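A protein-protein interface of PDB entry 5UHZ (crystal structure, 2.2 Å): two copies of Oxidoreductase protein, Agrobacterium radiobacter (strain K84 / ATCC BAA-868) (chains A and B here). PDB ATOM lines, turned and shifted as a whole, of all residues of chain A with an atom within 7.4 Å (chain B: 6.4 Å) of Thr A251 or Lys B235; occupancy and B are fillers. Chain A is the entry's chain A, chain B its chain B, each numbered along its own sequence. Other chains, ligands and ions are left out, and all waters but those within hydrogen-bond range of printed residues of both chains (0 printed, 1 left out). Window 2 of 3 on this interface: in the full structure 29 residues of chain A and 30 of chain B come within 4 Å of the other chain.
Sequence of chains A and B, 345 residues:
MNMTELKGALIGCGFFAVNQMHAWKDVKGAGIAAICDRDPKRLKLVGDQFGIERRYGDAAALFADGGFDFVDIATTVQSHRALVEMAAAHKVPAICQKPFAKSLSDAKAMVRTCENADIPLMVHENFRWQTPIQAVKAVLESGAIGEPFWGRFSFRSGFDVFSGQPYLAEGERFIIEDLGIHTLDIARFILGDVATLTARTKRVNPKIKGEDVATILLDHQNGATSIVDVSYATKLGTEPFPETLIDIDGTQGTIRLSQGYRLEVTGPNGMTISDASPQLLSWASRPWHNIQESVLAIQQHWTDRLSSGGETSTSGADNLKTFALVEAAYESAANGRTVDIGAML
The backbone carbonyl oxygen (O) of Ile A145 lies within hydrogen-bond range of the backbone NH (N) of Thr A251 (3.4 Å).
The backbone carbonyl oxygen (O) of Ile A145 is in hydrogen-bond range of the backbone NH (N) of Gly A253 (3.2 Å).
N of Thr A251 sits at hydrogen-bond distance from O of Glu A147, 3.0 Å away.
The backbone carbonyl oxygen (O) of Thr A254 lies within hydrogen-bond range of the backbone NH (N) of Thr A266, 2.9 Å away.
O of Ser B157 lies within hydrogen-bond range of N of Thr B234.
O of Thr B234 lies within hydrogen-bond range of N of Gly B158 (3.1 Å).
OG1 of Thr B234 lies within hydrogen-bond range of OD2 of Asp A249, at 2.7 Å.
The backbone carbonyl oxygen of Thr A251 sits at hydrogen-bond distance from the side-chain amino group of Lys B235, 3.2 Å away.
The backbone carbonyl oxygen (O) of Lys B235 lies within hydrogen-bond range of the side-chain hydroxyl (OG1) of Thr A254 (2.9 Å).
N of Gly B237 lies within hydrogen-bond range of OG1 of Thr A266, at 3.3 Å.
Thr A251 touches two residues of chain B.
Lys B235 touches five residues of chain A.
Printed residues of chain B within 4 Å of Arg A256: Thr B234 (3.6 Å) and Leu B236 (3.8 Å).
Printed residues of chain A within 4 Å of Gly B237: Thr A266.
Of the printed residues of chain B, Thr A254 touches Thr B234, Lys B235 and Leu B236.
Pro A268 touches none of the printed residues of chain B.
The nearest residue of chain B that does not touch Thr A251 is Ala B233 (5.6 Å).
The nearest residue of chain A that does not touch Lys B235 is Gly A250 (4.9 Å).
Phe A149 touches Val B204.
Val B204 touches Thr A251 (CG1 to CG2, 3.9 Å).
Gln A252 touches Lys B235 (C to CD, 3.6 Å).
Lys B235 touches Gly A253 (CD to N, 3.8 Å).
CG2 of Thr A254 touches CG2 of Thr B234, 3.7 Å away.
Leu B236 touches Thr A254 (CD2 to OG1, 3.7 Å).
CG2 of Thr B234 touches NH2 of Arg A256, at 3.6 Å.
Leu B236 touches Arg A256 (CD2 to NH2, 3.8 Å).
Thr A266 touches Lys B235 (CG2 to O, 3.6 Å).
C of Leu B236 touches CG2 of Thr A266 (3.96 Å).
Of the 9 printed residues of chain B, 6 touch a printed residue of chain A.
Of the 19 printed residues of chain A, 8 touch a printed residue of chain B.
Hydrophobic or aromatic side chains of chain A that line the printed part of chain B: Phe A149.
Among the printed residues, 15 pairs touch across the chains.
No position is printed for both chains.
Of the 15 pairs that touch across the chains among the printed residues, none has its exchanged pair printed and touching as well.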
ATOM      1  N   ILE A 145       1.452 -21.144 -12.132  1.00  0.00           N
ATOM      2  CA  ILE A 145       0.855 -21.726 -13.342  1.00  0.00           C
ATOM      3  C   ILE A 145      -0.469 -22.470 -13.114  1.00  0.00           C
ATOM      4  O   ILE A 145      -0.939 -23.176 -14.013  1.00  0.00           O
ATOM      5  CB  ILE A 145       1.855 -22.652 -14.065  1.00  0.00           C
ATOM      6  CG1 ILE A 145       2.211 -23.894 -13.231  1.00  0.00           C
ATOM      7  CG2 ILE A 145       3.109 -21.872 -14.419  1.00  0.00           C
ATOM      8  CD1 ILE A 145       2.818 -25.013 -14.056  1.00  0.00           C
ATOM      9  N   GLY A 146      -1.079 -22.292 -11.939  1.00  0.00           N
ATOM     10  CA  GLY A 146      -2.320 -22.984 -11.584  1.00  0.00           C
ATOM     11  C   GLY A 146      -2.108 -24.459 -11.287  1.00  0.00           C
ATOM     12  O   GLY A 146      -1.011 -24.870 -10.909  1.00  0.00           O
ATOM     13  N   GLU A 147      -3.172 -25.244 -11.456  1.00  0.00           N
ATOM     14  CA  GLU A 147      -3.132 -26.696 -11.257  1.00  0.00           C
ATOM     15  C   GLU A 147      -2.421 -27.368 -12.430  1.00  0.00           C
ATOM     16  O   GLU A 147      -2.826 -27.158 -13.574  1.00  0.00           O
ATOM     17  CB  GLU A 147      -4.550 -27.274 -11.167  1.00  0.00           C
ATOM     18  CG  GLU A 147      -5.348 -26.844  -9.941  1.00  0.00           C
ATOM     19  CD  GLU A 147      -4.940 -27.558  -8.658  1.00  0.00           C
ATOM     20  OE1 GLU A 147      -3.991 -28.382  -8.671  1.00  0.00           O
ATOM     21  OE2 GLU A 147      -5.581 -27.286  -7.621  1.00  0.00           O
ATOM     22  N   PRO A 148      -1.384 -28.192 -12.157  1.00  0.00           N
ATOM     23  CA  PRO A 148      -0.704 -28.900 -13.246  1.00  0.00           C
ATOM     24  C   PRO A 148      -1.569 -30.025 -13.829  1.00  0.00           C
ATOM     25  O   PRO A 148      -2.271 -30.705 -13.080  1.00  0.00           O
ATOM     26  CB  PRO A 148       0.538 -29.477 -12.560  1.00  0.00           C
ATOM     27  CG  PRO A 148       0.099 -29.705 -11.155  1.00  0.00           C
ATOM     28  CD  PRO A 148      -0.854 -28.590 -10.838  1.00  0.00           C
ATOM     29  N   PHE A 149      -1.536 -30.185 -15.152  1.00  0.00           N
ATOM     30  CA  PHE A 149      -2.221 -31.299 -15.830  1.00  0.00           C
ATOM     31  C   PHE A 149      -1.328 -32.180 -16.713  1.00  0.00           C
ATOM     32  O   PHE A 149      -1.740 -33.279 -17.078  1.00  0.00           O
ATOM     33  CB  PHE A 149      -3.430 -30.787 -16.636  1.00  0.00           C
ATOM     34  CG  PHE A 149      -3.077 -29.906 -17.814  1.00  0.00           C
ATOM     35  CD1 PHE A 149      -2.671 -30.461 -19.023  1.00  0.00           C
ATOM     36  CD2 PHE A 149      -3.208 -28.523 -17.729  1.00  0.00           C
ATOM     37  CE1 PHE A 149      -2.364 -29.655 -20.110  1.00  0.00           C
ATOM     38  CE2 PHE A 149      -2.912 -27.713 -18.816  1.00  0.00           C
ATOM     39  CZ  PHE A 149      -2.489 -28.279 -20.009  1.00  0.00           C
ATOM     40  N   TRP A 150      -0.140 -31.700 -17.083  1.00  0.00           N
ATOM     41  CA  TRP A 150       0.746 -32.445 -17.971  1.00  0.00           C
ATOM     42  C   TRP A 150       2.193 -32.145 -17.620  1.00  0.00           C
ATOM     43  O   TRP A 150       2.521 -31.017 -17.254  1.00  0.00           O
ATOM     44  CB  TRP A 150       0.464 -32.094 -19.443  1.00  0.00           C
ATOM     45  CG  TRP A 150       1.283 -32.885 -20.425  1.00  0.00           C
ATOM     46  CD1 TRP A 150       0.974 -34.099 -20.957  1.00  0.00           C
ATOM     47  CD2 TRP A 150       2.553 -32.516 -20.976  1.00  0.00           C
ATOM     48  NE1 TRP A 150       1.970 -34.512 -21.809  1.00  0.00           N
ATOM     49  CE2 TRP A 150       2.950 -33.556 -21.843  1.00  0.00           C
ATOM     50  CE3 TRP A 150       3.389 -31.398 -20.832  1.00  0.00           C
ATOM     51  CZ2 TRP A 150       4.150 -33.519 -22.561  1.00  0.00           C
ATOM     52  CZ3 TRP A 150       4.586 -31.359 -21.550  1.00  0.00           C
ATOM     53  CH2 TRP A 150       4.952 -32.414 -22.402  1.00  0.00           C
ATOM     54  N   ILE A 248       6.260 -28.553 -17.441  1.00  0.00           N
ATOM     55  CA  ILE A 248       4.976 -28.719 -16.785  1.00  0.00           C
ATOM     56  C   ILE A 248       3.987 -27.771 -17.443  1.00  0.00           C
ATOM     57  O   ILE A 248       4.324 -26.623 -17.691  1.00  0.00           O
ATOM     58  CB  ILE A 248       5.036 -28.425 -15.260  1.00  0.00           C
ATOM     59  CG1 ILE A 248       6.245 -29.094 -14.592  1.00  0.00           C
ATOM     60  CG2 ILE A 248       3.750 -28.880 -14.576  1.00  0.00           C
ATOM     61  CD1 ILE A 248       6.154 -30.602 -14.492  1.00  0.00           C
ATOM     62  N   ASP A 249       2.780 -28.256 -17.729  1.00  0.00           N
ATOM     63  CA  ASP A 249       1.689 -27.419 -18.230  1.00  0.00           C
ATOM     64  C   ASP A 249       0.590 -27.388 -17.186  1.00  0.00           C
ATOM     65  O   ASP A 249       0.143 -28.443 -16.727  1.00  0.00           O
ATOM     66  CB  ASP A 249       1.101 -27.980 -19.531  1.00  0.00           C
ATOM     67  CG  ASP A 249       2.023 -27.825 -20.724  1.00  0.00           C
ATOM     68  OD1 ASP A 249       3.172 -27.349 -20.572  1.00  0.00           O
ATOM     69  OD2 ASP A 249       1.585 -28.194 -21.829  1.00  0.00           O
ATOM     70  N   GLY A 250       0.156 -26.180 -16.827  1.00  0.00           N
ATOM     71  CA  GLY A 250      -0.919 -25.984 -15.869  1.00  0.00           C
ATOM     72  C   GLY A 250      -2.062 -25.187 -16.458  1.00  0.00           C
ATOM     73  O   GLY A 250      -1.951 -24.628 -17.549  1.00  0.00           O
ATOM     74  N   THR A 251      -3.157 -25.122 -15.707  1.00  0.00           N
ATOM     75  CA  THR A 251      -4.383 -24.425 -16.124  1.00  0.00           C
ATOM     76  C   THR A 251      -4.181 -22.929 -16.404  1.00  0.00           C
ATOM     77  O   THR A 251      -4.913 -22.352 -17.206  1.00  0.00           O
ATOM     78  CB  THR A 251      -5.496 -24.574 -15.058  1.00  0.00           C
ATOM     79  OG1 THR A 251      -4.983 -24.190 -13.775  1.00  0.00           O
ATOM     80  CG2 THR A 251      -6.006 -26.023 -14.986  1.00  0.00           C
ATOM     81  N   GLN A 252      -3.197 -22.317 -15.737  1.00  0.00           N
ATOM     82  CA  GLN A 252      -2.887 -20.892 -15.896  1.00  0.00           C
ATOM     83  C   GLN A 252      -1.469 -20.585 -16.424  1.00  0.00           C
ATOM     84  O   GLN A 252      -1.085 -19.415 -16.493  1.00  0.00           O
ATOM     85  CB  GLN A 252      -3.131 -20.186 -14.558  1.00  0.00           C
ATOM     86  CG  GLN A 252      -4.613 -20.045 -14.227  1.00  0.00           C
ATOM     87  CD  GLN A 252      -4.880 -19.557 -12.814  1.00  0.00           C
ATOM     88  OE1 GLN A 252      -4.005 -19.596 -11.946  1.00  0.00           O
ATOM     89  NE2 GLN A 252      -6.104 -19.098 -12.575  1.00  0.00           N
ATOM     90  N   GLY A 253      -0.702 -21.603 -16.818  1.00  0.00           N
ATOM     91  CA  GLY A 253       0.649 -21.360 -17.323  1.00  0.00           C
ATOM     92  C   GLY A 253       1.521 -22.572 -17.596  1.00  0.00           C
ATOM     93  O   GLY A 253       1.040 -23.705 -17.641  1.00  0.00           O
ATOM     94  N   THR A 254       2.817 -22.309 -17.770  1.00  0.00           N
ATOM     95  CA  THR A 254       3.811 -23.331 -18.096  1.00  0.00           C
ATOM     96  C   THR A 254       5.130 -23.091 -17.380  1.00  0.00           C
ATOM     97  O   THR A 254       5.512 -21.945 -17.129  1.00  0.00           O
ATOM     98  CB  THR A 254       4.148 -23.357 -19.606  1.00  0.00           C
ATOM     99  OG1 THR A 254       4.540 -22.049 -20.041  1.00  0.00           O
ATOM    100  CG2 THR A 254       2.961 -23.840 -20.425  1.00  0.00           C
ATOM    101  N   ILE A 255       5.811 -24.191 -17.066  1.00  0.00           N
ATOM    102  CA  ILE A 255       7.181 -24.186 -16.566  1.00  0.00           C
ATOM    103  C   ILE A 255       7.996 -24.935 -17.604  1.00  0.00           C
ATOM    104  O   ILE A 255       7.549 -25.963 -18.118  1.00  0.00           O
ATOM    105  CB  ILE A 255       7.313 -24.909 -15.208  1.00  0.00           C
ATOM    106  CG1 ILE A 255       6.479 -24.203 -14.139  1.00  0.00           C
ATOM    107  CG2 ILE A 255       8.775 -24.995 -14.774  1.00  0.00           C
ATOM    108  CD1 ILE A 255       6.155 -25.082 -12.952  1.00  0.00           C
ATOM    109  N   ARG A 256       9.175 -24.407 -17.923  1.00  0.00           N
ATOM    110  CA  ARG A 256      10.109 -25.068 -18.825  1.00  0.00           C
ATOM    111  C   ARG A 256      11.499 -24.940 -18.230  1.00  0.00           C
ATOM    112  O   ARG A 256      12.033 -23.840 -18.133  1.00  0.00           O
ATOM    113  CB  ARG A 256      10.054 -24.451 -20.229  1.00  0.00           C
ATOM    114  CG  ARG A 256       8.719 -24.639 -20.952  1.00  0.00           C
ATOM    115  CD  ARG A 256       8.470 -26.093 -21.328  1.00  0.00           C
ATOM    116  NE  ARG A 256       7.259 -26.276 -22.135  1.00  0.00           N
ATOM    117  CZ  ARG A 256       6.023 -26.479 -21.666  1.00  0.00           C
ATOM    118  NH1 ARG A 256       5.761 -26.523 -20.357  1.00  0.00           N
ATOM    119  NH2 ARG A 256       5.023 -26.643 -22.525  1.00  0.00           N
ATOM    120  N   VAL A 265       9.134 -19.496 -16.815  1.00  0.00           N
ATOM    121  CA  VAL A 265       7.825 -19.619 -16.197  1.00  0.00           C
ATOM    122  C   VAL A 265       6.922 -18.607 -16.862  1.00  0.00           C
ATOM    123  O   VAL A 265       7.266 -17.432 -16.920  1.00  0.00           O
ATOM    124  CB  VAL A 265       7.895 -19.342 -14.678  1.00  0.00           C
ATOM    125  CG1 VAL A 265       6.499 -19.368 -14.054  1.00  0.00           C
ATOM    126  CG2 VAL A 265       8.813 -20.361 -14.013  1.00  0.00           C
ATOM    127  N   THR A 266       5.782 -19.065 -17.372  1.00  0.00           N
ATOM    128  CA  THR A 266       4.777 -18.177 -17.949  1.00  0.00           C
ATOM    129  C   THR A 266       3.509 -18.279 -17.116  1.00  0.00           C
ATOM    130  O   THR A 266       3.096 -19.373 -16.750  1.00  0.00           O
ATOM    131  CB  THR A 266       4.492 -18.528 -19.418  1.00  0.00           C
ATOM    132  OG1 THR A 266       5.692 -18.356 -20.181  1.00  0.00           O
ATOM    133  CG2 THR A 266       3.396 -17.631 -20.001  1.00  0.00           C
ATOM    134  N   GLY A 267       2.912 -17.128 -16.822  1.00  0.00           N
ATOM    135  CA  GLY A 267       1.699 -17.045 -16.014  1.00  0.00           C
ATOM    136  C   GLY A 267       0.781 -15.935 -16.492  1.00  0.00           C
ATOM    137  O   GLY A 267       1.082 -15.268 -17.483  1.00  0.00           O
ATOM    138  N   PRO A 268      -0.350 -15.730 -15.788  1.00  0.00           N
ATOM    139  CA  PRO A 268      -1.317 -14.686 -16.156  1.00  0.00           C
ATOM    140  C   PRO A 268      -0.700 -13.288 -16.301  1.00  0.00           C
ATOM    141  O   PRO A 268      -1.161 -12.502 -17.134  1.00  0.00           O
ATOM    142  CB  PRO A 268      -2.321 -14.710 -14.995  1.00  0.00           C
ATOM    143  CG  PRO A 268      -2.210 -16.080 -14.421  1.00  0.00           C
ATOM    144  CD  PRO A 268      -0.768 -16.459 -14.574  1.00  0.00           C
ATOM    145  N   SER B 157       0.026 -25.702 -27.928  1.00  0.00           N
ATOM    146  CA  SER B 157      -0.397 -24.354 -28.294  1.00  0.00           C
ATOM    147  C   SER B 157      -1.462 -23.828 -27.334  1.00  0.00           C
ATOM    148  O   SER B 157      -2.089 -24.593 -26.603  1.00  0.00           O
ATOM    149  CB  SER B 157      -0.960 -24.375 -29.720  1.00  0.00           C
ATOM    150  OG  SER B 157      -1.532 -23.132 -30.094  1.00  0.00           O
ATOM    151  N   GLY B 158      -1.637 -22.509 -27.332  1.00  0.00           N
ATOM    152  CA  GLY B 158      -2.750 -21.850 -26.645  1.00  0.00           C
ATOM    153  C   GLY B 158      -3.522 -20.930 -27.574  1.00  0.00           C
ATOM    154  O   GLY B 158      -4.191 -20.007 -27.118  1.00  0.00           O
ATOM    155  N   VAL B 204      -9.160 -29.512 -20.336  1.00  0.00           N
ATOM    156  CA  VAL B 204      -8.760 -28.420 -19.447  1.00  0.00           C
ATOM    157  C   VAL B 204      -9.637 -27.181 -19.658  1.00  0.00           C
ATOM    158  O   VAL B 204     -10.125 -26.599 -18.690  1.00  0.00           O
ATOM    159  CB  VAL B 204      -7.267 -28.068 -19.643  1.00  0.00           C
ATOM    160  CG1 VAL B 204      -6.853 -26.906 -18.741  1.00  0.00           C
ATOM    161  CG2 VAL B 204      -6.403 -29.295 -19.367  1.00  0.00           C
ATOM    162  N   ALA B 233      -4.279 -26.246 -24.662  1.00  0.00           N
ATOM    163  CA  ALA B 233      -4.379 -25.564 -23.365  1.00  0.00           C
ATOM    164  C   ALA B 233      -3.002 -25.276 -22.758  1.00  0.00           C
ATOM    165  O   ALA B 233      -2.870 -25.185 -21.534  1.00  0.00           O
ATOM    166  CB  ALA B 233      -5.212 -26.397 -22.405  1.00  0.00           C
ATOM    167  N   THR B 234      -1.992 -25.119 -23.620  1.00  0.00           N
ATOM    168  CA  THR B 234      -0.615 -24.838 -23.204  1.00  0.00           C
ATOM    169  C   THR B 234      -0.310 -23.349 -23.416  1.00  0.00           C
ATOM    170  O   THR B 234      -0.245 -22.877 -24.553  1.00  0.00           O
ATOM    171  CB  THR B 234       0.388 -25.716 -23.983  1.00  0.00           C
ATOM    172  OG1 THR B 234       0.075 -27.099 -23.768  1.00  0.00           O
ATOM    173  CG2 THR B 234       1.810 -25.463 -23.530  1.00  0.00           C
ATOM    174  N   LYS B 235      -0.132 -22.627 -22.308  1.00  0.00           N
ATOM    175  CA  LYS B 235       0.089 -21.180 -22.312  1.00  0.00           C
ATOM    176  C   LYS B 235       1.582 -20.871 -22.229  1.00  0.00           C
ATOM    177  O   LYS B 235       2.166 -20.872 -21.141  1.00  0.00           O
ATOM    178  CB  LYS B 235      -0.638 -20.536 -21.129  1.00  0.00           C
ATOM    179  CG  LYS B 235      -2.152 -20.680 -21.140  1.00  0.00           C
ATOM    180  CD  LYS B 235      -2.721 -20.359 -19.762  1.00  0.00           C
ATOM    181  CE  LYS B 235      -4.221 -20.108 -19.801  1.00  0.00           C
ATOM    182  NZ  LYS B 235      -4.981 -21.293 -20.275  1.00  0.00           N
ATOM    183  N   LEU B 236       2.187 -20.602 -23.384  1.00  0.00           N
ATOM    184  CA  LEU B 236       3.620 -20.334 -23.494  1.00  0.00           C
ATOM    185  C   LEU B 236       3.897 -18.856 -23.738  1.00  0.00           C
ATOM    186  O   LEU B 236       3.029 -18.125 -24.210  1.00  0.00           O
ATOM    187  CB  LEU B 236       4.214 -21.151 -24.640  1.00  0.00           C
ATOM    188  CG  LEU B 236       4.343 -22.656 -24.394  1.00  0.00           C
ATOM    189  CD1 LEU B 236       4.488 -23.402 -25.713  1.00  0.00           C
ATOM    190  CD2 LEU B 236       5.512 -22.968 -23.471  1.00  0.00           C
ATOM    191  N   GLY B 237       5.121 -18.438 -23.422  1.00  0.00           N
ATOM    192  CA  GLY B 237       5.575 -17.064 -23.650  1.00  0.00           C
ATOM    193  C   GLY B 237       5.768 -16.697 -25.115  1.00  0.00           C
ATOM    194  O   GLY B 237       5.707 -15.519 -25.474  1.00  0.00           O
ATOM    195  N   GLU B 239       4.093 -18.096 -28.628  1.00  0.00           N
ATOM    196  CA  GLU B 239       3.063 -18.975 -29.189  1.00  0.00           C
ATOM    197  C   GLU B 239       3.571 -19.688 -30.453  1.00  0.00           C
ATOM    198  O   GLU B 239       3.812 -19.028 -31.462  1.00  0.00           O
ATOM    199  CB  GLU B 239       1.790 -18.163 -29.512  1.00  0.00           C
ATOM    200  CG  GLU B 239       0.649 -18.940 -30.168  1.00  0.00           C
ATOM    201  CD  GLU B 239       0.294 -20.218 -29.425  1.00  0.00           C
ATOM    202  OE1 GLU B 239      -0.109 -20.128 -28.245  1.00  0.00           O
ATOM    203  OE2 GLU B 239       0.416 -21.315 -30.019  1.00  0.00           O
